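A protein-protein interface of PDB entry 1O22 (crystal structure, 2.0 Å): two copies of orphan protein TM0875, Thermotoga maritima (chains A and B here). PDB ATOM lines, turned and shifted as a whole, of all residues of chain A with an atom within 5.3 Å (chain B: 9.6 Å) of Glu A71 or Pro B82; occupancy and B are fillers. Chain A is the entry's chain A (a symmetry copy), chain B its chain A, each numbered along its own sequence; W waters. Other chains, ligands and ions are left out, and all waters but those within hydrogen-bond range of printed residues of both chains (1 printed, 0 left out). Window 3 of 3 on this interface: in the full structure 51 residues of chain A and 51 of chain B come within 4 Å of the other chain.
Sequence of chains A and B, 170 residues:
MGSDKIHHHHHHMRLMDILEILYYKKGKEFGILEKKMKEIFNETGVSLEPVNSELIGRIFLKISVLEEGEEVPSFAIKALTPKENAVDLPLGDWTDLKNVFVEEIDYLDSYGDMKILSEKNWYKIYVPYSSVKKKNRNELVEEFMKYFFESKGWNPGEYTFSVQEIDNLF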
ATOM      1  N   LEU A  66      35.249  -4.887  -2.542  1.00  0.00           N
ATOM      2  CA  LEU A  66      33.879  -5.140  -2.992  1.00  0.00           C
ATOM      3  C   LEU A  66      33.681  -4.408  -4.294  1.00  0.00           C
ATOM      4  O   LEU A  66      34.182  -3.323  -4.467  1.00  0.00           O
ATOM      5  CB  LEU A  66      32.883  -4.659  -1.932  1.00  0.00           C
ATOM      6  CG  LEU A  66      33.199  -5.332  -0.573  1.00  0.00           C
ATOM      7  CD1 LEU A  66      32.862  -4.392   0.564  1.00  0.00           C
ATOM      8  CD2 LEU A  66      32.500  -6.642  -0.476  1.00  0.00           C
ATOM      9  N   GLY A  69      28.584  -1.046  -6.628  1.00  0.00           N
ATOM     10  CA  GLY A  69      27.194  -1.422  -6.511  1.00  0.00           C
ATOM     11  C   GLY A  69      26.968  -2.544  -5.491  1.00  0.00           C
ATOM     12  O   GLY A  69      25.867  -3.066  -5.415  1.00  0.00           O
ATOM     13  N   GLU A  70      28.013  -2.902  -4.729  1.00  0.00           N
ATOM     14  CA  GLU A  70      27.924  -3.845  -3.613  1.00  0.00           C
ATOM     15  C   GLU A  70      28.212  -3.152  -2.276  1.00  0.00           C
ATOM     16  O   GLU A  70      29.204  -2.416  -2.103  1.00  0.00           O
ATOM     17  CB  GLU A  70      28.888  -5.038  -3.807  1.00  0.00           C
ATOM     18  CG  GLU A  70      28.645  -5.858  -5.067  1.00  0.00           C
ATOM     19  CD  GLU A  70      29.628  -7.031  -5.218  1.00  0.00           C
ATOM     20  OE1 GLU A  70      30.557  -7.177  -4.377  1.00  0.00           O
ATOM     21  OE2 GLU A  70      29.468  -7.809  -6.197  1.00  0.00           O
ATOM     22  N   GLU A  71      27.341  -3.448  -1.320  1.00  0.00           N
ATOM     23  CA  GLU A  71      27.508  -3.105   0.105  1.00  0.00           C
ATOM     24  C   GLU A  71      28.548  -3.915   0.823  1.00  0.00           C
ATOM     25  O   GLU A  71      28.727  -5.096   0.516  1.00  0.00           O
ATOM     26  CB  GLU A  71      26.191  -3.329   0.821  1.00  0.00           C
ATOM     27  CG  GLU A  71      25.108  -2.390   0.374  1.00  0.00           C
ATOM     28  CD  GLU A  71      23.793  -2.627   1.088  1.00  0.00           C
ATOM     29  OE1 GLU A  71      23.181  -3.685   0.863  1.00  0.00           O
ATOM     30  OE2 GLU A  71      23.359  -1.734   1.840  1.00  0.00           O
ATOM     31  N   VAL A  72      29.241  -3.274   1.760  1.00  0.00           N
ATOM     32  CA  VAL A  72      30.159  -3.964   2.663  1.00  0.00           C
ATOM     33  C   VAL A  72      29.353  -4.840   3.622  1.00  0.00           C
ATOM     34  O   VAL A  72      28.227  -4.526   3.947  1.00  0.00           O
ATOM     35  CB  VAL A  72      31.072  -2.970   3.521  1.00  0.00           C
ATOM     36  CG1 VAL A  72      31.988  -2.146   2.618  1.00  0.00           C
ATOM     37  CG2 VAL A  72      30.235  -2.071   4.481  1.00  0.00           C
ATOM     38  N   PRO A  73      29.933  -5.942   4.033  1.00  0.00           N
ATOM     39  CA  PRO A  73      29.298  -6.821   4.999  1.00  0.00           C
ATOM     40  C   PRO A  73      29.283  -6.199   6.400  1.00  0.00           C
ATOM     41  O   PRO A  73      30.159  -5.456   6.785  1.00  0.00           O
ATOM     42  CB  PRO A  73      30.205  -8.063   4.968  1.00  0.00           C
ATOM     43  CG  PRO A  73      31.518  -7.596   4.493  1.00  0.00           C
ATOM     44  CD  PRO A  73      31.274  -6.411   3.628  1.00  0.00           C
ATOM     45  N   SER A  74      28.234  -6.474   7.139  1.00  0.00           N
ATOM     46  CA  SER A  74      28.215  -6.249   8.566  1.00  0.00           C
ATOM     47  C   SER A  74      28.362  -7.501   9.398  1.00  0.00           C
ATOM     48  O   SER A  74      28.782  -7.389  10.530  1.00  0.00           O
ATOM     49  CB  SER A  74      26.920  -5.547   8.964  1.00  0.00           C
ATOM     50  OG  SER A  74      26.898  -4.257   8.419  1.00  0.00           O
ATOM     51  N   TRP A  94      27.284 -13.399  -4.863  1.00  0.00           N
ATOM     52  CA  TRP A  94      26.006 -13.387  -4.154  1.00  0.00           C
ATOM     53  C   TRP A  94      25.108 -14.543  -4.604  1.00  0.00           C
ATOM     54  O   TRP A  94      25.190 -15.017  -5.751  1.00  0.00           O
ATOM     55  CB  TRP A  94      25.315 -12.011  -4.329  1.00  0.00           C
ATOM     56  CG  TRP A  94      26.218 -10.859  -3.840  1.00  0.00           C
ATOM     57  CD1 TRP A  94      27.265 -10.290  -4.519  1.00  0.00           C
ATOM     58  CD2 TRP A  94      26.178 -10.194  -2.557  1.00  0.00           C
ATOM     59  NE1 TRP A  94      27.873  -9.327  -3.747  1.00  0.00           N
ATOM     60  CE2 TRP A  94      27.227  -9.245  -2.540  1.00  0.00           C
ATOM     61  CE3 TRP A  94      25.373 -10.314  -1.426  1.00  0.00           C
ATOM     62  CZ2 TRP A  94      27.475  -8.418  -1.448  1.00  0.00           C
ATOM     63  CZ3 TRP A  94      25.615  -9.498  -0.344  1.00  0.00           C
ATOM     64  CH2 TRP A  94      26.663  -8.565  -0.354  1.00  0.00           C
ATOM     65  N   ALA B  79      29.541 -17.131   4.634  1.00  0.00           N
ATOM     66  CA  ALA B  79      28.737 -16.154   3.911  1.00  0.00           C
ATOM     67  C   ALA B  79      28.811 -14.792   4.617  1.00  0.00           C
ATOM     68  O   ALA B  79      28.937 -14.715   5.828  1.00  0.00           O
ATOM     69  CB  ALA B  79      27.302 -16.633   3.871  1.00  0.00           C
ATOM     70  N   LEU B  80      28.656 -13.713   3.891  1.00  0.00           N
ATOM     71  CA  LEU B  80      28.610 -12.393   4.525  1.00  0.00           C
ATOM     72  C   LEU B  80      27.285 -11.743   4.145  1.00  0.00           C
ATOM     73  O   LEU B  80      26.822 -11.854   3.016  1.00  0.00           O
ATOM     74  CB  LEU B  80      29.788 -11.534   4.030  1.00  0.00           C
ATOM     75  CG  LEU B  80      31.196 -12.119   4.095  1.00  0.00           C
ATOM     76  CD1 LEU B  80      32.130 -11.452   3.139  1.00  0.00           C
ATOM     77  CD2 LEU B  80      31.721 -11.963   5.523  1.00  0.00           C
ATOM     78  N   THR B  81      26.689 -11.046   5.087  1.00  0.00           N
ATOM     79  CA  THR B  81      25.519 -10.239   4.835  1.00  0.00           C
ATOM     80  C   THR B  81      25.751  -8.752   5.123  1.00  0.00           C
ATOM     81  O   THR B  81      26.402  -8.431   6.094  1.00  0.00           O
ATOM     82  CB  THR B  81      24.361 -10.835   5.687  1.00  0.00           C
ATOM     83  OG1 THR B  81      23.227  -9.998   5.558  1.00  0.00           O
ATOM     84  CG2 THR B  81      24.710 -10.857   7.151  1.00  0.00           C
ATOM     85  N   PRO B  82      25.210  -7.849   4.293  1.00  0.00           N
ATOM     86  CA  PRO B  82      25.235  -6.410   4.551  1.00  0.00           C
ATOM     87  C   PRO B  82      24.154  -5.925   5.479  1.00  0.00           C
ATOM     88  O   PRO B  82      24.155  -4.737   5.768  1.00  0.00           O
ATOM     89  CB  PRO B  82      24.985  -5.805   3.161  1.00  0.00           C
ATOM     90  CG  PRO B  82      24.225  -6.845   2.424  1.00  0.00           C
ATOM     91  CD  PRO B  82      24.587  -8.140   2.989  1.00  0.00           C
ATOM     92  N   LYS B  83      23.239  -6.812   5.892  1.00  0.00           N
ATOM     93  CA  LYS B  83      22.192  -6.460   6.825  1.00  0.00           C
ATOM     94  C   LYS B  83      22.797  -5.942   8.124  1.00  0.00           C
ATOM     95  O   LYS B  83      23.748  -6.510   8.628  1.00  0.00           O
ATOM     96  CB  LYS B  83      21.321  -7.681   7.091  1.00  0.00           C
ATOM     97  CG  LYS B  83      20.228  -7.915   6.065  1.00  0.00           C
ATOM     98  CD  LYS B  83      18.917  -8.430   6.735  1.00  0.00           C
ATOM     99  CE  LYS B  83      18.283  -7.423   7.710  1.00  0.00           C
ATOM    100  NZ  LYS B  83      17.540  -8.076   8.838  1.00  0.00           N
ATOM    101  N   GLU B  84      22.231  -4.897   8.693  1.00  0.00           N
ATOM    102  CA  GLU B  84      22.867  -4.237   9.843  1.00  0.00           C
ATOM    103  C   GLU B  84      22.472  -4.794  11.214  1.00  0.00           C
ATOM    104  O   GLU B  84      23.041  -4.421  12.224  1.00  0.00           O
ATOM    105  CB  GLU B  84      22.660  -2.729   9.773  1.00  0.00           C
ATOM    106  CG  GLU B  84      23.501  -2.114   8.665  1.00  0.00           C
ATOM    107  CD  GLU B  84      23.235  -0.642   8.447  1.00  0.00           C
ATOM    108  OE1 GLU B  84      22.380  -0.061   9.156  1.00  0.00           O
ATOM    109  OE2 GLU B  84      23.895  -0.066   7.556  1.00  0.00           O
ATOM    110  N   ASN B  85      21.525  -5.719  11.243  1.00  0.00           N
ATOM    111  CA  ASN B  85      21.310  -6.516  12.449  1.00  0.00           C
ATOM    112  C   ASN B  85      21.145  -7.996  12.136  1.00  0.00           C
ATOM    113  O   ASN B  85      20.859  -8.379  11.011  1.00  0.00           O
ATOM    114  CB  ASN B  85      20.155  -5.963  13.229  1.00  0.00           C
ATOM    115  CG  ASN B  85      18.880  -6.162  12.549  1.00  0.00           C
ATOM    116  OD1 ASN B  85      18.397  -7.293  12.469  1.00  0.00           O
ATOM    117  ND2 ASN B  85      18.274  -5.071  12.089  1.00  0.00           N
ATOM    118  N   ALA B  86      21.381  -8.793  13.159  1.00  0.00           N
ATOM    119  CA  ALA B  86      21.344 -10.233  13.113  1.00  0.00           C
ATOM    120  C   ALA B  86      20.181 -10.845  13.904  1.00  0.00           C
ATOM    121  O   ALA B  86      20.152 -12.062  14.150  1.00  0.00           O
ATOM    122  CB  ALA B  86      22.652 -10.771  13.634  1.00  0.00           C
ATOM    123  N   ASP B  88      17.303 -11.620  13.071  1.00  0.00           N
ATOM    124  CA  ASP B  88      16.586 -12.676  12.341  1.00  0.00           C
ATOM    125  C   ASP B  88      17.364 -13.990  12.120  1.00  0.00           C
ATOM    126  O   ASP B  88      16.838 -14.917  11.522  1.00  0.00           O
ATOM    127  CB  ASP B  88      16.072 -12.151  11.008  1.00  0.00           C
ATOM    128  CG  ASP B  88      17.180 -11.822  10.033  1.00  0.00           C
ATOM    129  OD1 ASP B  88      18.344 -11.660  10.469  1.00  0.00           O
ATOM    130  OD2 ASP B  88      16.973 -11.689   8.804  1.00  0.00           O
ATOM    131  N   LEU B  89      18.601 -14.060  12.608  1.00  0.00           N
ATOM    132  CA  LEU B  89      19.476 -15.205  12.416  1.00  0.00           C
ATOM    133  C   LEU B  89      19.572 -16.027  13.698  1.00  0.00           C
ATOM    134  O   LEU B  89      19.988 -15.481  14.740  1.00  0.00           O
ATOM    135  CB  LEU B  89      20.908 -14.727  12.063  1.00  0.00           C
ATOM    136  CG  LEU B  89      21.109 -13.875  10.811  1.00  0.00           C
ATOM    137  CD1 LEU B  89      22.564 -13.341  10.675  1.00  0.00           C
ATOM    138  CD2 LEU B  89      20.721 -14.646   9.576  1.00  0.00           C
ATOM    139  N   LYS B  98      18.784 -15.273   2.533  1.00  0.00           N
ATOM    140  CA  LYS B  98      18.603 -14.551   1.275  1.00  0.00           C
ATOM    141  C   LYS B  98      19.716 -13.550   1.015  1.00  0.00           C
ATOM    142  O   LYS B  98      20.098 -12.807   1.903  1.00  0.00           O
ATOM    143  CB  LYS B  98      17.259 -13.801   1.275  1.00  0.00           C
ATOM    144  N   ASN B  99      20.218 -13.521  -0.219  1.00  0.00           N
ATOM    145  CA  ASN B  99      21.141 -12.482  -0.672  1.00  0.00           C
ATOM    146  C   ASN B  99      22.395 -12.357   0.217  1.00  0.00           C
ATOM    147  O   ASN B  99      22.674 -11.313   0.836  1.00  0.00           O
ATOM    148  CB  ASN B  99      20.431 -11.134  -0.797  1.00  0.00           C
ATOM    149  CG  ASN B  99      21.234 -10.133  -1.620  1.00  0.00           C
ATOM    150  OD1 ASN B  99      21.664 -10.452  -2.731  1.00  0.00           O
ATOM    151  ND2 ASN B  99      21.476  -8.941  -1.061  1.00  0.00           N
ATOM    152  N   VAL B 100      23.156 -13.442   0.268  1.00  0.00           N
ATOM    153  CA  VAL B 100      24.404 -13.434   0.987  1.00  0.00           C
ATOM    154  C   VAL B 100      25.548 -13.630   0.025  1.00  0.00           C
ATOM    155  O   VAL B 100      25.385 -14.230  -1.036  1.00  0.00           O
ATOM    156  CB  VAL B 100      24.391 -14.464   2.146  1.00  0.00           C
ATOM    157  CG1 VAL B 100      23.465 -13.985   3.241  1.00  0.00           C
ATOM    158  CG2 VAL B 100      23.973 -15.815   1.695  1.00  0.00           C
ATOM    159  N   PHE B 101      26.700 -13.086   0.383  1.00  0.00           N
ATOM    160  CA  PHE B 101      27.930 -13.276  -0.348  1.00  0.00           C
ATOM    161  C   PHE B 101      28.690 -14.505   0.164  1.00  0.00           C
ATOM    162  O   PHE B 101      29.108 -14.549   1.313  1.00  0.00           O
ATOM    163  CB  PHE B 101      28.785 -12.028  -0.236  1.00  0.00           C
ATOM    164  CG  PHE B 101      30.028 -12.065  -1.056  1.00  0.00           C
ATOM    165  CD1 PHE B 101      30.002 -11.674  -2.363  1.00  0.00           C
ATOM    166  CD2 PHE B 101      31.231 -12.464  -0.498  1.00  0.00           C
ATOM    167  CE1 PHE B 101      31.151 -11.672  -3.135  1.00  0.00           C
ATOM    168  CE2 PHE B 101      32.395 -12.467  -1.253  1.00  0.00           C
ATOM    169  CZ  PHE B 101      32.354 -12.067  -2.579  1.00  0.00           C
ATOM    170  N   VAL B 102      28.883 -15.496  -0.708  1.00  0.00           N
ATOM    171  CA  VAL B 102      29.681 -16.667  -0.370  1.00  0.00           C
ATOM    172  C   VAL B 102      31.147 -16.425  -0.522  1.00  0.00           C
ATOM    173  O   VAL B 102      31.633 -16.204  -1.604  1.00  0.00           O
ATOM    174  CB  VAL B 102      29.295 -17.851  -1.218  1.00  0.00           C
ATOM    175  CG1 VAL B 102      30.160 -19.100  -0.831  1.00  0.00           C
ATOM    176  CG2 VAL B 102      27.837 -18.126  -1.083  1.00  0.00           C
HETATM  177  O   HOH W   1      26.609  -3.503   6.085  1.00  0.00           O
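N of Leu B80 lies within hydrogen-bond range of O of Phe B101 (2.7 Å).
The side-chain hydroxyl (OG1) of Thr B81 lies within hydrogen-bond range of the backbone NH (N) of Lys B83, at 3.2 Å.
NZ of Lys B83 is in salt-bridge range of OD2 of Asp B88.
The indole nitrogen of Trp A94 lies close to the side-chain carboxylate of Glu A70 (3.3 Å).
Water W1 lies within hydrogen-bond range of OG of Ser A74 (2.5 Å), O of Pro B82 (2.8 Å) and O of Val A72 (2.9 Å).
The backbone NH (N) of Ser A74 lies within hydrogen-bond range of the backbone carbonyl oxygen (O) of Thr B81, 2.9 Å away.
Among the printed residues, pairs that only touch across the chains: Trp A94 with Val B100 (3.3 Å), Ser A74 with Lys B83 (3.3 Å), Trp A94 with Phe B101 (3.5 Å), Pro A73 with Thr B81 (3.5 Å), Val A72 with Pro B82 (3.6 Å), Glu A71 with Pro B82 (3.6 Å), Pro A73 with Leu B80 (3.6 Å), Trp A94 with Asn B99 (3.7 Å), Trp A94 with Pro B82 (3.7 Å) and Ser A74 with Pro B82 (3.8 Å).
Printed residues of chain B that touch a printed residue of chain A: Leu B80, Thr B81, Pro B82, Lys B83, Asn B99, Val B100 and Phe B101.
Among the printed residues, no Asp or Glu carboxylate lies within 4 Å of a Lys or Arg side-chain nitrogen of the other chain.
Of chain B, only Pro B82 (3.6 Å) comes within 4 Å of Glu A71.
Val A72 touches just one residue of chain B: Pro B82.
Of the printed residues of chain B, Trp A94 touches Pro B82 (3.7 Å), Asn B99 (3.7 Å), Val B100 (3.3 Å) and Phe B101 (3.5 Å).
Of the printed residues of chain A, Thr B81 touches Pro A73 and Ser A74.
Of chain A, only Glu A71 (3.6 Å), Val A72 (3.6 Å), Ser A74 (3.8 Å) and Trp A94 (3.7 Å) come within 4 Å of Pro B82.
Printed residues of chain A within 4 Å of Lys B83: Ser A74 (3.3 Å).
Printed residues of chain A within 4 Å of Asn B99: Trp A94 (3.7 Å).
Printed residues of chain A within 4 Å of Val B100: Trp A94 (3.3 Å).
The nearest residue of chain B that does not touch Glu A71 is Asn B99 (5.9 Å).
The nearest residue of chain A that does not touch Pro B82 is Pro A73 (4.1 Å).
No position is printed for both chains.
Of the 11 pairs that touch across the chains among the printed residues, none has its exchanged pair printed and touching as well.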
